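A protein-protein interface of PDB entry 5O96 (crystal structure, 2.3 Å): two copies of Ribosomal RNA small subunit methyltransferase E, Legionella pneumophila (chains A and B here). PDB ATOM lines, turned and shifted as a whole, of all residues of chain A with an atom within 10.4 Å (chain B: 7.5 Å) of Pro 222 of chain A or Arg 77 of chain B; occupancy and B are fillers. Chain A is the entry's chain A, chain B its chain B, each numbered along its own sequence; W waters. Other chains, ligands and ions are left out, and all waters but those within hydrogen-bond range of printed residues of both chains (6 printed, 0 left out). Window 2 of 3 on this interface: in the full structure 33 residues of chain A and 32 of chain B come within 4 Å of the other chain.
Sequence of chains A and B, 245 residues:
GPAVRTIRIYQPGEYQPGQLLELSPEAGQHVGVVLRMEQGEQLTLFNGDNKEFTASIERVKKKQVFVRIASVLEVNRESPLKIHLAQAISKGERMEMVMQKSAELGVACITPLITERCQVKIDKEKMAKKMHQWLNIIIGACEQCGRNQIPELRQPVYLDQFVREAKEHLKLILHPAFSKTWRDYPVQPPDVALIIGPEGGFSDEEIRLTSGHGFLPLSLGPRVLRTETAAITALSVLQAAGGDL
O of Arg 77 of chain B sits at hydrogen-bond distance from NH1 of Arg 223 of chain A (3.1 Å). The guanidinium group of Arg 223 of chain A sits at hydrogen-bond distance from the backbone carbonyl oxygen of Glu 104 of chain B (3.2 Å). NH1 of Arg 223 of chain A is in salt-bridge range of OD2 of Asp 244 of chain B. N of Val 224 of chain A sits at hydrogen-bond distance from O of Cys 145 of chain B (2.8 Å). The backbone NH (N) of Arg 226 of chain A sits at hydrogen-bond distance from the side-chain carboxylate (OE1) of Glu 104 of chain B (3.0 Å).
The guanidinium group of Arg 8 of chain B sits at hydrogen-bond distance from the backbone carbonyl oxygen of Arg 147 of chain B. NH1 of Arg 147 of chain B sits at hydrogen-bond distance from O of Ala 103 of chain B, at 3.1 Å. The backbone carbonyl oxygen of Cys 142 of chain B sits at hydrogen-bond distance from the backbone NH of Arg 147 of chain B (3.4 Å).
Among the printed residues, merely in contact across the chains: Gly 221 of chain A with Asp 244 of chain B (3.2 Å), Pro 222 of chain A with Asp 244 of chain B (3.3 Å), Arg 223 of chain A with Arg 147 of chain B (3.4 Å), Arg 223 of chain A with Gly 106 of chain B (3.5 Å), Arg 223 of chain A with Cys 145 of chain B (3.5 Å), Leu 220 of chain A with Leu 245 of chain B (3.6 Å), Val 224 of chain A with Arg 5 of chain B (3.6 Å), Arg 223 of chain A with Leu 105 of chain B (3.6 Å), Pro 222 of chain A with Arg 77 of chain B (3.6 Å), Leu 225 of chain A with Glu 104 of chain B (3.7 Å), Thr 233 of chain A with Leu 245 of chain B (3.7 Å), Thr 233 of chain A with Leu 105 of chain B (3.7 Å), Thr 181 of chain A with Leu 245 of chain B (3.7 Å), Arg 223 of chain A with Leu 245 of chain B (3.7 Å), Arg 223 of chain A with Ser 79 of chain B (3.8 Å) and Gly 221 of chain A with Leu 245 of chain B (3.96 Å).
Arg 77 of chain B touches just these residues of chain A: Pro 222 and Arg 223. Asn 76 of chain B touches none of the printed residues of chain A. No residue of chain A comes within 4 Å of Glu 78 of chain B. No residue of chain A comes within 4 Å of Gly 146 of chain B. Of the printed residues of chain B, Val 224 of chain A touches Arg 5 and Cys 145. Printed residues of chain A within 4 Å of Glu 104 of chain B: Arg 223, Leu 225 and Arg 226. Of the printed residues of chain A, Ser 79 of chain B touches Arg 223. Leu 174 of chain A touches none of the printed residues of chain B. The nearest residue of chain B that does not touch Pro 222 of chain A is Cys 145 of chain B (4.9 Å). The nearest residue of chain A that does not touch Arg 77 of chain B is Val 224 of chain A (6.0 Å).
Of the 24 printed residues of chain B, 10 touch a printed residue of chain A. Of the 14 printed residues of chain A, 9 touch a printed residue of chain B. Hydrophobic or aromatic side chains of chain A within 4 Å of the printed part of chain B: Pro 222, Val 224 and Leu 225.
No position is printed for both chains. Of the 21 pairs that touch across the chains among the printed residues, none has its exchanged pair printed and touching as well.
Water W2 bridges the backbone carbonyl oxygen of Pro 222 of chain A and the guanidinium group of Arg 77 of chain B. Water W3 lies within hydrogen-bond range of OXT of Leu 245 of chain B (2.7 Å), N of Gly 221 of chain A (2.8 Å) and OG of Ser 219 of chain A (2.9 Å). Water W1 lies within hydrogen-bond range of OG1 of Thr 181 of chain A (2.9 Å) and O of Leu 245 of chain B (3.0 Å).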
ATOM      1  N   LEU A 174     -30.970  -0.004  10.558  1.00  0.00           N
ATOM      2  CA  LEU A 174     -30.372   0.614  11.741  1.00  0.00           C
ATOM      3  C   LEU A 174     -29.313   1.607  11.276  1.00  0.00           C
ATOM      4  O   LEU A 174     -28.243   1.215  10.790  1.00  0.00           O
ATOM      5  CB  LEU A 174     -29.785  -0.443  12.676  1.00  0.00           C
ATOM      6  CG  LEU A 174     -29.113   0.127  13.911  1.00  0.00           C
ATOM      7  CD1 LEU A 174     -30.087   0.970  14.723  1.00  0.00           C
ATOM      8  CD2 LEU A 174     -28.565  -0.990  14.750  1.00  0.00           C
ATOM      9  N   PRO A 176     -28.272   6.101  12.060  1.00  0.00           N
ATOM     10  CA  PRO A 176     -28.647   7.277  12.861  1.00  0.00           C
ATOM     11  C   PRO A 176     -29.331   8.394  12.087  1.00  0.00           C
ATOM     12  O   PRO A 176     -30.149   9.109  12.677  1.00  0.00           O
ATOM     13  CB  PRO A 176     -27.294   7.761  13.412  1.00  0.00           C
ATOM     14  CG  PRO A 176     -26.337   6.653  13.171  1.00  0.00           C
ATOM     15  CD  PRO A 176     -26.814   5.913  11.976  1.00  0.00           C
ATOM     16  N   SER A 179     -33.131   9.223  11.788  1.00  0.00           N
ATOM     17  CA  SER A 179     -33.726   8.031  12.377  1.00  0.00           C
ATOM     18  C   SER A 179     -34.897   8.364  13.307  1.00  0.00           C
ATOM     19  O   SER A 179     -34.997   9.453  13.883  1.00  0.00           O
ATOM     20  CB  SER A 179     -32.678   7.253  13.164  1.00  0.00           C
ATOM     21  OG  SER A 179     -32.286   7.976  14.318  1.00  0.00           O
ATOM     22  N   THR A 181     -37.519   6.340  16.439  1.00  0.00           N
ATOM     23  CA  THR A 181     -37.575   5.193  17.328  1.00  0.00           C
ATOM     24  C   THR A 181     -38.674   4.255  16.889  1.00  0.00           C
ATOM     25  O   THR A 181     -39.494   4.571  16.018  1.00  0.00           O
ATOM     26  CB  THR A 181     -37.823   5.609  18.773  1.00  0.00           C
ATOM     27  OG1 THR A 181     -39.191   6.012  18.907  1.00  0.00           O
ATOM     28  CG2 THR A 181     -36.934   6.771  19.142  1.00  0.00           C
ATOM     29  N   LEU A 218     -34.069   3.457  11.640  1.00  0.00           N
ATOM     30  CA  LEU A 218     -34.428   3.150  13.017  1.00  0.00           C
ATOM     31  C   LEU A 218     -33.251   3.422  13.952  1.00  0.00           C
ATOM     32  O   LEU A 218     -32.144   2.948  13.692  1.00  0.00           O
ATOM     33  CB  LEU A 218     -34.815   1.674  13.122  1.00  0.00           C
ATOM     34  CG  LEU A 218     -35.058   1.161  14.551  1.00  0.00           C
ATOM     35  CD1 LEU A 218     -36.424   1.659  14.941  1.00  0.00           C
ATOM     36  CD2 LEU A 218     -34.915  -0.390  14.645  1.00  0.00           C
ATOM     37  N   SER A 219     -33.492   4.144  15.046  1.00  0.00           N
ATOM     38  CA  SER A 219     -32.494   4.317  16.105  1.00  0.00           C
ATOM     39  C   SER A 219     -32.723   3.348  17.264  1.00  0.00           C
ATOM     40  O   SER A 219     -33.838   2.851  17.495  1.00  0.00           O
ATOM     41  CB  SER A 219     -32.515   5.740  16.647  1.00  0.00           C
ATOM     42  OG  SER A 219     -33.842   6.052  17.061  1.00  0.00           O
ATOM     43  N   LEU A 220     -31.649   3.113  18.027  1.00  0.00           N
ATOM     44  CA  LEU A 220     -31.712   2.310  19.248  1.00  0.00           C
ATOM     45  C   LEU A 220     -30.952   3.023  20.367  1.00  0.00           C
ATOM     46  O   LEU A 220     -30.051   2.472  20.991  1.00  0.00           O
ATOM     47  CB  LEU A 220     -31.177   0.887  19.043  1.00  0.00           C
ATOM     48  CG  LEU A 220     -32.009   0.054  18.054  1.00  0.00           C
ATOM     49  CD1 LEU A 220     -31.296  -1.238  17.740  1.00  0.00           C
ATOM     50  CD2 LEU A 220     -33.384  -0.250  18.625  1.00  0.00           C
ATOM     51  N   GLY A 221     -31.360   4.256  20.646  1.00  0.00           N
ATOM     52  CA  GLY A 221     -30.779   5.033  21.715  1.00  0.00           C
ATOM     53  C   GLY A 221     -29.559   5.816  21.273  1.00  0.00           C
ATOM     54  O   GLY A 221     -29.051   5.647  20.165  1.00  0.00           O
ATOM     55  N   PRO A 222     -29.044   6.659  22.168  1.00  0.00           N
ATOM     56  CA  PRO A 222     -27.950   7.577  21.827  1.00  0.00           C
ATOM     57  C   PRO A 222     -26.566   6.978  21.953  1.00  0.00           C
ATOM     58  O   PRO A 222     -25.587   7.701  21.749  1.00  0.00           O
ATOM     59  CB  PRO A 222     -28.127   8.689  22.863  1.00  0.00           C
ATOM     60  CG  PRO A 222     -28.701   7.958  24.086  1.00  0.00           C
ATOM     61  CD  PRO A 222     -29.562   6.879  23.537  1.00  0.00           C
ATOM     62  N   ARG A 223     -26.463   5.699  22.271  1.00  0.00           N
ATOM     63  CA  ARG A 223     -25.178   5.069  22.510  1.00  0.00           C
ATOM     64  C   ARG A 223     -24.841   4.169  21.331  1.00  0.00           C
ATOM     65  O   ARG A 223     -25.699   3.424  20.840  1.00  0.00           O
ATOM     66  CB  ARG A 223     -25.194   4.266  23.833  1.00  0.00           C
ATOM     67  CG  ARG A 223     -25.279   5.134  25.107  1.00  0.00           C
ATOM     68  CD  ARG A 223     -25.603   4.252  26.384  1.00  0.00           C
ATOM     69  NE  ARG A 223     -26.865   3.536  26.235  1.00  0.00           N
ATOM     70  CZ  ARG A 223     -28.053   4.080  26.502  1.00  0.00           C
ATOM     71  NH1 ARG A 223     -28.121   5.326  26.956  1.00  0.00           N
ATOM     72  NH2 ARG A 223     -29.176   3.386  26.318  1.00  0.00           N
ATOM     73  N   VAL A 224     -23.582   4.199  20.898  1.00  0.00           N
ATOM     74  CA  VAL A 224     -23.198   3.352  19.780  1.00  0.00           C
ATOM     75  C   VAL A 224     -23.153   1.895  20.221  1.00  0.00           C
ATOM     76  O   VAL A 224     -22.356   1.510  21.070  1.00  0.00           O
ATOM     77  CB  VAL A 224     -21.859   3.796  19.196  1.00  0.00           C
ATOM     78  CG1 VAL A 224     -21.469   2.866  18.061  1.00  0.00           C
ATOM     79  CG2 VAL A 224     -21.992   5.219  18.738  1.00  0.00           C
ATOM     80  N   LEU A 225     -24.002   1.075  19.626  1.00  0.00           N
ATOM     81  CA  LEU A 225     -24.013  -0.344  19.939  1.00  0.00           C
ATOM     82  C   LEU A 225     -23.048  -1.111  19.039  1.00  0.00           C
ATOM     83  O   LEU A 225     -22.876  -0.788  17.866  1.00  0.00           O
ATOM     84  CB  LEU A 225     -25.422  -0.912  19.782  1.00  0.00           C
ATOM     85  CG  LEU A 225     -26.589  -0.255  20.514  1.00  0.00           C
ATOM     86  CD1 LEU A 225     -27.887  -0.988  20.155  1.00  0.00           C
ATOM     87  CD2 LEU A 225     -26.369  -0.232  22.026  1.00  0.00           C
ATOM     88  N   ARG A 226     -22.417  -2.144  19.593  1.00  0.00           N
ATOM     89  CA  ARG A 226     -21.682  -3.050  18.725  1.00  0.00           C
ATOM     90  C   ARG A 226     -22.621  -3.690  17.696  1.00  0.00           C
ATOM     91  O   ARG A 226     -23.842  -3.744  17.866  1.00  0.00           O
ATOM     92  CB  ARG A 226     -20.973  -4.138  19.524  1.00  0.00           C
ATOM     93  CG  ARG A 226     -19.874  -3.643  20.439  1.00  0.00           C
ATOM     94  CD  ARG A 226     -19.151  -4.834  21.046  1.00  0.00           C
ATOM     95  NE  ARG A 226     -17.935  -4.443  21.746  1.00  0.00           N
ATOM     96  CZ  ARG A 226     -16.745  -4.370  21.162  1.00  0.00           C
ATOM     97  NH1 ARG A 226     -16.612  -4.668  19.876  1.00  0.00           N
ATOM     98  NH2 ARG A 226     -15.690  -4.006  21.870  1.00  0.00           N
ATOM     99  N   THR A 233     -30.584  -6.441  20.329  1.00  0.00           N
ATOM    100  CA  THR A 233     -31.391  -5.303  20.773  1.00  0.00           C
ATOM    101  C   THR A 233     -32.523  -4.997  19.793  1.00  0.00           C
ATOM    102  O   THR A 233     -33.677  -4.837  20.191  1.00  0.00           O
ATOM    103  CB  THR A 233     -30.472  -4.100  20.942  1.00  0.00           C
ATOM    104  OG1 THR A 233     -29.527  -4.401  21.976  1.00  0.00           O
ATOM    105  CG2 THR A 233     -31.258  -2.862  21.298  1.00  0.00           C
ATOM    106  N   ARG B   5     -14.117   8.830  14.142  1.00  0.00           N
ATOM    107  CA  ARG B   5     -14.200   9.493  15.437  1.00  0.00           C
ATOM    108  C   ARG B   5     -12.998   9.155  16.313  1.00  0.00           C
ATOM    109  O   ARG B   5     -12.461   8.046  16.275  1.00  0.00           O
ATOM    110  CB  ARG B   5     -15.486   9.099  16.162  1.00  0.00           C
ATOM    111  CG  ARG B   5     -16.644  10.069  15.952  1.00  0.00           C
ATOM    112  CD  ARG B   5     -17.885   9.585  16.674  1.00  0.00           C
ATOM    113  NE  ARG B   5     -17.816   8.144  16.918  1.00  0.00           N
ATOM    114  CZ  ARG B   5     -18.839   7.398  17.324  1.00  0.00           C
ATOM    115  NH1 ARG B   5     -20.027   7.959  17.523  1.00  0.00           N
ATOM    116  NH2 ARG B   5     -18.668   6.092  17.520  1.00  0.00           N
ATOM    117  N   ARG B   8     -11.651   7.054  22.328  1.00  0.00           N
ATOM    118  CA  ARG B   8     -12.155   7.390  23.660  1.00  0.00           C
ATOM    119  C   ARG B   8     -11.422   6.579  24.720  1.00  0.00           C
ATOM    120  O   ARG B   8     -11.315   5.355  24.599  1.00  0.00           O
ATOM    121  CB  ARG B   8     -13.657   7.121  23.752  1.00  0.00           C
ATOM    122  CG  ARG B   8     -14.525   8.091  22.987  1.00  0.00           C
ATOM    123  CD  ARG B   8     -15.934   7.515  22.842  1.00  0.00           C
ATOM    124  NE  ARG B   8     -16.469   7.152  24.160  1.00  0.00           N
ATOM    125  CZ  ARG B   8     -16.934   8.027  25.062  1.00  0.00           C
ATOM    126  NH1 ARG B   8     -16.936   9.310  24.801  1.00  0.00           N
ATOM    127  NH2 ARG B   8     -17.388   7.625  26.256  1.00  0.00           N
ATOM    128  N   THR B  44      -9.884  11.408  23.061  1.00  0.00           N
ATOM    129  CA  THR B  44     -11.003  11.913  23.841  1.00  0.00           C
ATOM    130  C   THR B  44     -10.964  11.188  25.176  1.00  0.00           C
ATOM    131  O   THR B  44     -11.259   9.993  25.241  1.00  0.00           O
ATOM    132  CB  THR B  44     -12.350  11.697  23.157  1.00  0.00           C
ATOM    133  OG1 THR B  44     -12.353  12.393  21.908  1.00  0.00           O
ATOM    134  CG2 THR B  44     -13.487  12.223  24.077  1.00  0.00           C
ATOM    135  N   ASN B  50     -19.585  12.783  32.892  1.00  0.00           N
ATOM    136  CA  ASN B  50     -20.257  13.290  31.680  1.00  0.00           C
ATOM    137  C   ASN B  50     -19.520  14.503  31.084  1.00  0.00           C
ATOM    138  O   ASN B  50     -20.104  15.520  30.703  1.00  0.00           O
ATOM    139  CB  ASN B  50     -21.740  13.554  31.979  1.00  0.00           C
ATOM    140  CG  ASN B  50     -22.471  12.244  32.305  1.00  0.00           C
ATOM    141  OD1 ASN B  50     -22.384  11.298  31.535  1.00  0.00           O
ATOM    142  ND2 ASN B  50     -23.083  12.152  33.487  1.00  0.00           N
ATOM    143  N   GLU B  52     -16.168  15.153  28.248  1.00  0.00           N
ATOM    144  CA  GLU B  52     -15.241  14.665  27.233  1.00  0.00           C
ATOM    145  C   GLU B  52     -14.148  15.711  27.102  1.00  0.00           C
ATOM    146  O   GLU B  52     -14.440  16.894  26.873  1.00  0.00           O
ATOM    147  CB  GLU B  52     -15.927  14.447  25.883  1.00  0.00           C
ATOM    148  CG  GLU B  52     -16.998  13.369  25.894  1.00  0.00           C
ATOM    149  CD  GLU B  52     -17.506  13.031  24.480  1.00  0.00           C
ATOM    150  OE1 GLU B  52     -17.071  13.708  23.542  1.00  0.00           O
ATOM    151  OE2 GLU B  52     -18.284  12.058  24.308  1.00  0.00           O
ATOM    152  N   VAL B  75     -21.102  16.204  27.927  1.00  0.00           N
ATOM    153  CA  VAL B  75     -21.800  15.307  27.021  1.00  0.00           C
ATOM    154  C   VAL B  75     -22.311  14.137  27.831  1.00  0.00           C
ATOM    155  O   VAL B  75     -21.515  13.367  28.375  1.00  0.00           O
ATOM    156  CB  VAL B  75     -20.868  14.796  25.900  1.00  0.00           C
ATOM    157  CG1 VAL B  75     -21.549  13.746  25.087  1.00  0.00           C
ATOM    158  CG2 VAL B  75     -20.377  15.947  25.006  1.00  0.00           C
ATOM    159  N   ASN B  76     -23.625  13.949  27.843  1.00  0.00           N
ATOM    160  CA  ASN B  76     -24.290  12.968  28.692  1.00  0.00           C
ATOM    161  C   ASN B  76     -25.046  12.015  27.783  1.00  0.00           C
ATOM    162  O   ASN B  76     -25.931  12.447  27.045  1.00  0.00           O
ATOM    163  CB  ASN B  76     -25.232  13.692  29.675  1.00  0.00           C
ATOM    164  CG  ASN B  76     -26.039  12.740  30.573  1.00  0.00           C
ATOM    165  OD1 ASN B  76     -26.481  11.660  30.175  1.00  0.00           O
ATOM    166  ND2 ASN B  76     -26.258  13.181  31.806  1.00  0.00           N
ATOM    167  N   ARG B  77     -24.702  10.736  27.830  1.00  0.00           N
ATOM    168  CA  ARG B  77     -25.410   9.707  27.074  1.00  0.00           C
ATOM    169  C   ARG B  77     -26.014   8.665  28.013  1.00  0.00           C
ATOM    170  O   ARG B  77     -26.029   7.462  27.721  1.00  0.00           O
ATOM    171  CB  ARG B  77     -24.490   9.048  26.042  1.00  0.00           C
ATOM    172  CG  ARG B  77     -24.000  10.023  24.951  1.00  0.00           C
ATOM    173  CD  ARG B  77     -23.163   9.370  23.857  1.00  0.00           C
ATOM    174  NE  ARG B  77     -22.674  10.343  22.870  1.00  0.00           N
ATOM    175  CZ  ARG B  77     -21.463  10.912  22.846  1.00  0.00           C
ATOM    176  NH1 ARG B  77     -20.535  10.639  23.753  1.00  0.00           N
ATOM    177  NH2 ARG B  77     -21.158  11.780  21.889  1.00  0.00           N
ATOM    178  N   GLU B  78     -26.531   9.120  29.154  1.00  0.00           N
ATOM    179  CA  GLU B  78     -27.164   8.233  30.111  1.00  0.00           C
ATOM    180  C   GLU B  78     -28.672   8.156  29.885  1.00  0.00           C
ATOM    181  O   GLU B  78     -29.332   9.131  29.496  1.00  0.00           O
ATOM    182  CB  GLU B  78     -26.865   8.716  31.537  1.00  0.00           C
ATOM    183  CG  GLU B  78     -25.380   8.736  31.841  1.00  0.00           C
ATOM    184  CD  GLU B  78     -24.786   7.371  31.706  1.00  0.00           C
ATOM    185  OE1 GLU B  78     -25.274   6.482  32.426  1.00  0.00           O
ATOM    186  OE2 GLU B  78     -23.877   7.159  30.871  1.00  0.00           O
ATOM    187  N   SER B  79     -29.220   6.979  30.144  1.00  0.00           N
ATOM    188  CA  SER B  79     -30.645   6.821  30.011  1.00  0.00           C
ATOM    189  C   SER B  79     -31.344   7.527  31.167  1.00  0.00           C
ATOM    190  O   SER B  79     -30.808   7.605  32.277  1.00  0.00           O
ATOM    191  CB  SER B  79     -31.008   5.350  29.982  1.00  0.00           C
ATOM    192  OG  SER B  79     -32.397   5.225  29.930  1.00  0.00           O
ATOM    193  N   PRO B  80     -32.519   8.101  30.927  1.00  0.00           N
ATOM    194  CA  PRO B  80     -33.244   8.740  32.033  1.00  0.00           C
ATOM    195  C   PRO B  80     -33.910   7.731  32.930  1.00  0.00           C
ATOM    196  O   PRO B  80     -34.314   8.086  34.048  1.00  0.00           O
ATOM    197  CB  PRO B  80     -34.282   9.611  31.309  1.00  0.00           C
ATOM    198  CG  PRO B  80     -34.584   8.811  30.052  1.00  0.00           C
ATOM    199  CD  PRO B  80     -33.248   8.216  29.641  1.00  0.00           C
ATOM    200  N   ALA B 103     -23.643  -2.532  29.924  1.00  0.00           N
ATOM    201  CA  ALA B 103     -23.116  -1.171  29.865  1.00  0.00           C
ATOM    202  C   ALA B 103     -23.439  -0.507  28.517  1.00  0.00           C
ATOM    203  O   ALA B 103     -23.853   0.658  28.483  1.00  0.00           O
ATOM    204  CB  ALA B 103     -21.608  -1.177  30.133  1.00  0.00           C
ATOM    205  N   GLU B 104     -23.302  -1.244  27.401  1.00  0.00           N
ATOM    206  CA  GLU B 104     -23.723  -0.693  26.107  1.00  0.00           C
ATOM    207  C   GLU B 104     -25.174  -0.256  26.130  1.00  0.00           C
ATOM    208  O   GLU B 104     -25.530   0.721  25.454  1.00  0.00           O
ATOM    209  CB  GLU B 104     -23.549  -1.692  24.966  1.00  0.00           C
ATOM    210  CG  GLU B 104     -22.163  -2.129  24.660  1.00  0.00           C
ATOM    211  CD  GLU B 104     -22.140  -3.119  23.520  1.00  0.00           C
ATOM    212  OE1 GLU B 104     -22.789  -2.845  22.521  1.00  0.00           O
ATOM    213  OE2 GLU B 104     -21.473  -4.171  23.614  1.00  0.00           O
ATOM    214  N   LEU B 105     -26.017  -0.958  26.907  1.00  0.00           N
ATOM    215  CA  LEU B 105     -27.450  -0.701  26.972  1.00  0.00           C
ATOM    216  C   LEU B 105     -27.852   0.287  28.068  1.00  0.00           C
ATOM    217  O   LEU B 105     -29.051   0.429  28.351  1.00  0.00           O
ATOM    218  CB  LEU B 105     -28.209  -2.026  27.140  1.00  0.00           C
ATOM    219  CG  LEU B 105     -28.204  -2.780  25.811  1.00  0.00           C
ATOM    220  CD1 LEU B 105     -28.468  -4.264  26.000  1.00  0.00           C
ATOM    221  CD2 LEU B 105     -29.229  -2.161  24.875  1.00  0.00           C
ATOM    222  N   GLY B 106     -26.895   0.979  28.681  1.00  0.00           N
ATOM    223  CA  GLY B 106     -27.233   2.099  29.529  1.00  0.00           C
ATOM    224  C   GLY B 106     -27.565   1.749  30.962  1.00  0.00           C
ATOM    225  O   GLY B 106     -28.033   2.637  31.696  1.00  0.00           O
ATOM    226  N   CYS B 142     -17.980   1.447  27.950  1.00  0.00           N
ATOM    227  CA  CYS B 142     -18.272   2.871  27.914  1.00  0.00           C
ATOM    228  C   CYS B 142     -17.373   3.583  26.901  1.00  0.00           C
ATOM    229  O   CYS B 142     -17.820   4.521  26.227  1.00  0.00           O
ATOM    230  CB  CYS B 142     -18.149   3.471  29.315  1.00  0.00           C
ATOM    231  SG  CYS B 142     -19.257   2.616  30.555  1.00  0.00           S
ATOM    232  N   CYS B 145     -18.991   2.621  23.477  1.00  0.00           N
ATOM    233  CA  CYS B 145     -20.357   3.017  23.142  1.00  0.00           C
ATOM    234  C   CYS B 145     -20.646   4.501  23.357  1.00  0.00           C
ATOM    235  O   CYS B 145     -21.645   5.002  22.816  1.00  0.00           O
ATOM    236  CB  CYS B 145     -21.394   2.176  23.907  1.00  0.00           C
ATOM    237  SG  CYS B 145     -21.695   2.644  25.636  1.00  0.00           S
ATOM    238  N   GLY B 146     -19.799   5.225  24.095  1.00  0.00           N
ATOM    239  CA  GLY B 146     -19.928   6.666  24.240  1.00  0.00           C
ATOM    240  C   GLY B 146     -20.487   7.149  25.565  1.00  0.00           C
ATOM    241  O   GLY B 146     -20.678   8.356  25.716  1.00  0.00           O
ATOM    242  N   ARG B 147     -20.757   6.256  26.524  1.00  0.00           N
ATOM    243  CA  ARG B 147     -21.114   6.688  27.882  1.00  0.00           C
ATOM    244  C   ARG B 147     -19.930   7.354  28.556  1.00  0.00           C
ATOM    245  O   ARG B 147     -18.835   6.795  28.602  1.00  0.00           O
ATOM    246  CB  ARG B 147     -21.568   5.510  28.748  1.00  0.00           C
ATOM    247  CG  ARG B 147     -22.846   4.833  28.310  1.00  0.00           C
ATOM    248  CD  ARG B 147     -23.215   3.707  29.265  1.00  0.00           C
ATOM    249  NE  ARG B 147     -23.604   4.179  30.598  1.00  0.00           N
ATOM    250  CZ  ARG B 147     -24.092   3.375  31.523  1.00  0.00           C
ATOM    251  NH1 ARG B 147     -24.250   2.093  31.216  1.00  0.00           N
ATOM    252  NH2 ARG B 147     -24.455   3.842  32.728  1.00  0.00           N
ATOM    253  N   ASN B 148     -20.149   8.551  29.084  1.00  0.00           N
ATOM    254  CA  ASN B 148     -19.120   9.281  29.805  1.00  0.00           C
ATOM    255  C   ASN B 148     -19.314   9.159  31.310  1.00  0.00           C
ATOM    256  O   ASN B 148     -18.869  10.018  32.080  1.00  0.00           O
ATOM    257  CB  ASN B 148     -19.129  10.736  29.344  1.00  0.00           C
ATOM    258  CG  ASN B 148     -18.806  10.850  27.871  1.00  0.00           C
ATOM    259  OD1 ASN B 148     -17.980  10.088  27.365  1.00  0.00           O
ATOM    260  ND2 ASN B 148     -19.505  11.729  27.161  1.00  0.00           N
ATOM    261  N   GLN B 149     -20.024   8.115  31.725  1.00  0.00           N
ATOM    262  CA  GLN B 149     -20.291   7.825  33.124  1.00  0.00           C
ATOM    263  C   GLN B 149     -20.307   6.311  33.230  1.00  0.00           C
ATOM    264  O   GLN B 149     -20.972   5.643  32.430  1.00  0.00           O
ATOM    265  CB  GLN B 149     -21.637   8.446  33.592  1.00  0.00           C
ATOM    266  CG  GLN B 149     -22.030   8.061  35.005  1.00  0.00           C
ATOM    267  CD  GLN B 149     -23.326   8.705  35.494  1.00  0.00           C
ATOM    268  OE1 GLN B 149     -23.847   9.637  34.904  1.00  0.00           O
ATOM    269  NE2 GLN B 149     -23.832   8.206  36.600  1.00  0.00           N
ATOM    270  N   GLY B 243     -37.007   4.201  28.762  1.00  0.00           N
ATOM    271  CA  GLY B 243     -35.704   4.858  28.752  1.00  0.00           C
ATOM    272  C   GLY B 243     -35.481   5.687  27.498  1.00  0.00           C
ATOM    273  O   GLY B 243     -36.341   6.507  27.145  1.00  0.00           O
ATOM    274  N   ASP B 244     -34.355   5.497  26.801  1.00  0.00           N
ATOM    275  CA  ASP B 244     -34.036   6.339  25.650  1.00  0.00           C
ATOM    276  C   ASP B 244     -33.885   5.542  24.356  1.00  0.00           C
ATOM    277  O   ASP B 244     -33.331   6.056  23.377  1.00  0.00           O
ATOM    278  CB  ASP B 244     -32.796   7.195  25.928  1.00  0.00           C
ATOM    279  CG  ASP B 244     -31.575   6.376  26.374  1.00  0.00           C
ATOM    280  OD1 ASP B 244     -31.651   5.138  26.414  1.00  0.00           O
ATOM    281  OD2 ASP B 244     -30.538   6.991  26.702  1.00  0.00           O
ATOM    282  N   LEU B 245     -34.416   4.319  24.310  1.00  0.00           N
ATOM    283  CA  LEU B 245     -34.375   3.507  23.096  1.00  0.00           C
ATOM    284  C   LEU B 245     -35.626   3.721  22.261  1.00  0.00           C
ATOM    285  O   LEU B 245     -36.718   3.864  22.812  1.00  0.00           O
ATOM    286  CB  LEU B 245     -34.230   2.022  23.410  1.00  0.00           C
ATOM    287  CG  LEU B 245     -32.843   1.487  23.074  1.00  0.00           C
ATOM    288  CD1 LEU B 245     -31.796   2.031  24.081  1.00  0.00           C
ATOM    289  CD2 LEU B 245     -32.836  -0.019  23.005  1.00  0.00           C
ATOM    290  OXT LEU B 245     -35.561   3.750  21.020  1.00  0.00           O
HETATM  291  O   HOH W   1     -39.083   5.383  21.779  1.00  0.00           O
HETATM  292  O   HOH W   2     -24.914  10.205  21.310  1.00  0.00           O
HETATM  293  O   HOH W   3     -33.753   5.459  19.859  1.00  0.00           O
HETATM  294  O   HOH W   4     -18.730  -2.610  23.857  1.00  0.00           O
HETATM  295  O   HOH W   5     -28.027   1.619  24.595  1.00  0.00           O
HETATM  296  O   HOH W   6     -36.111   2.507  18.808  1.00  0.00           O
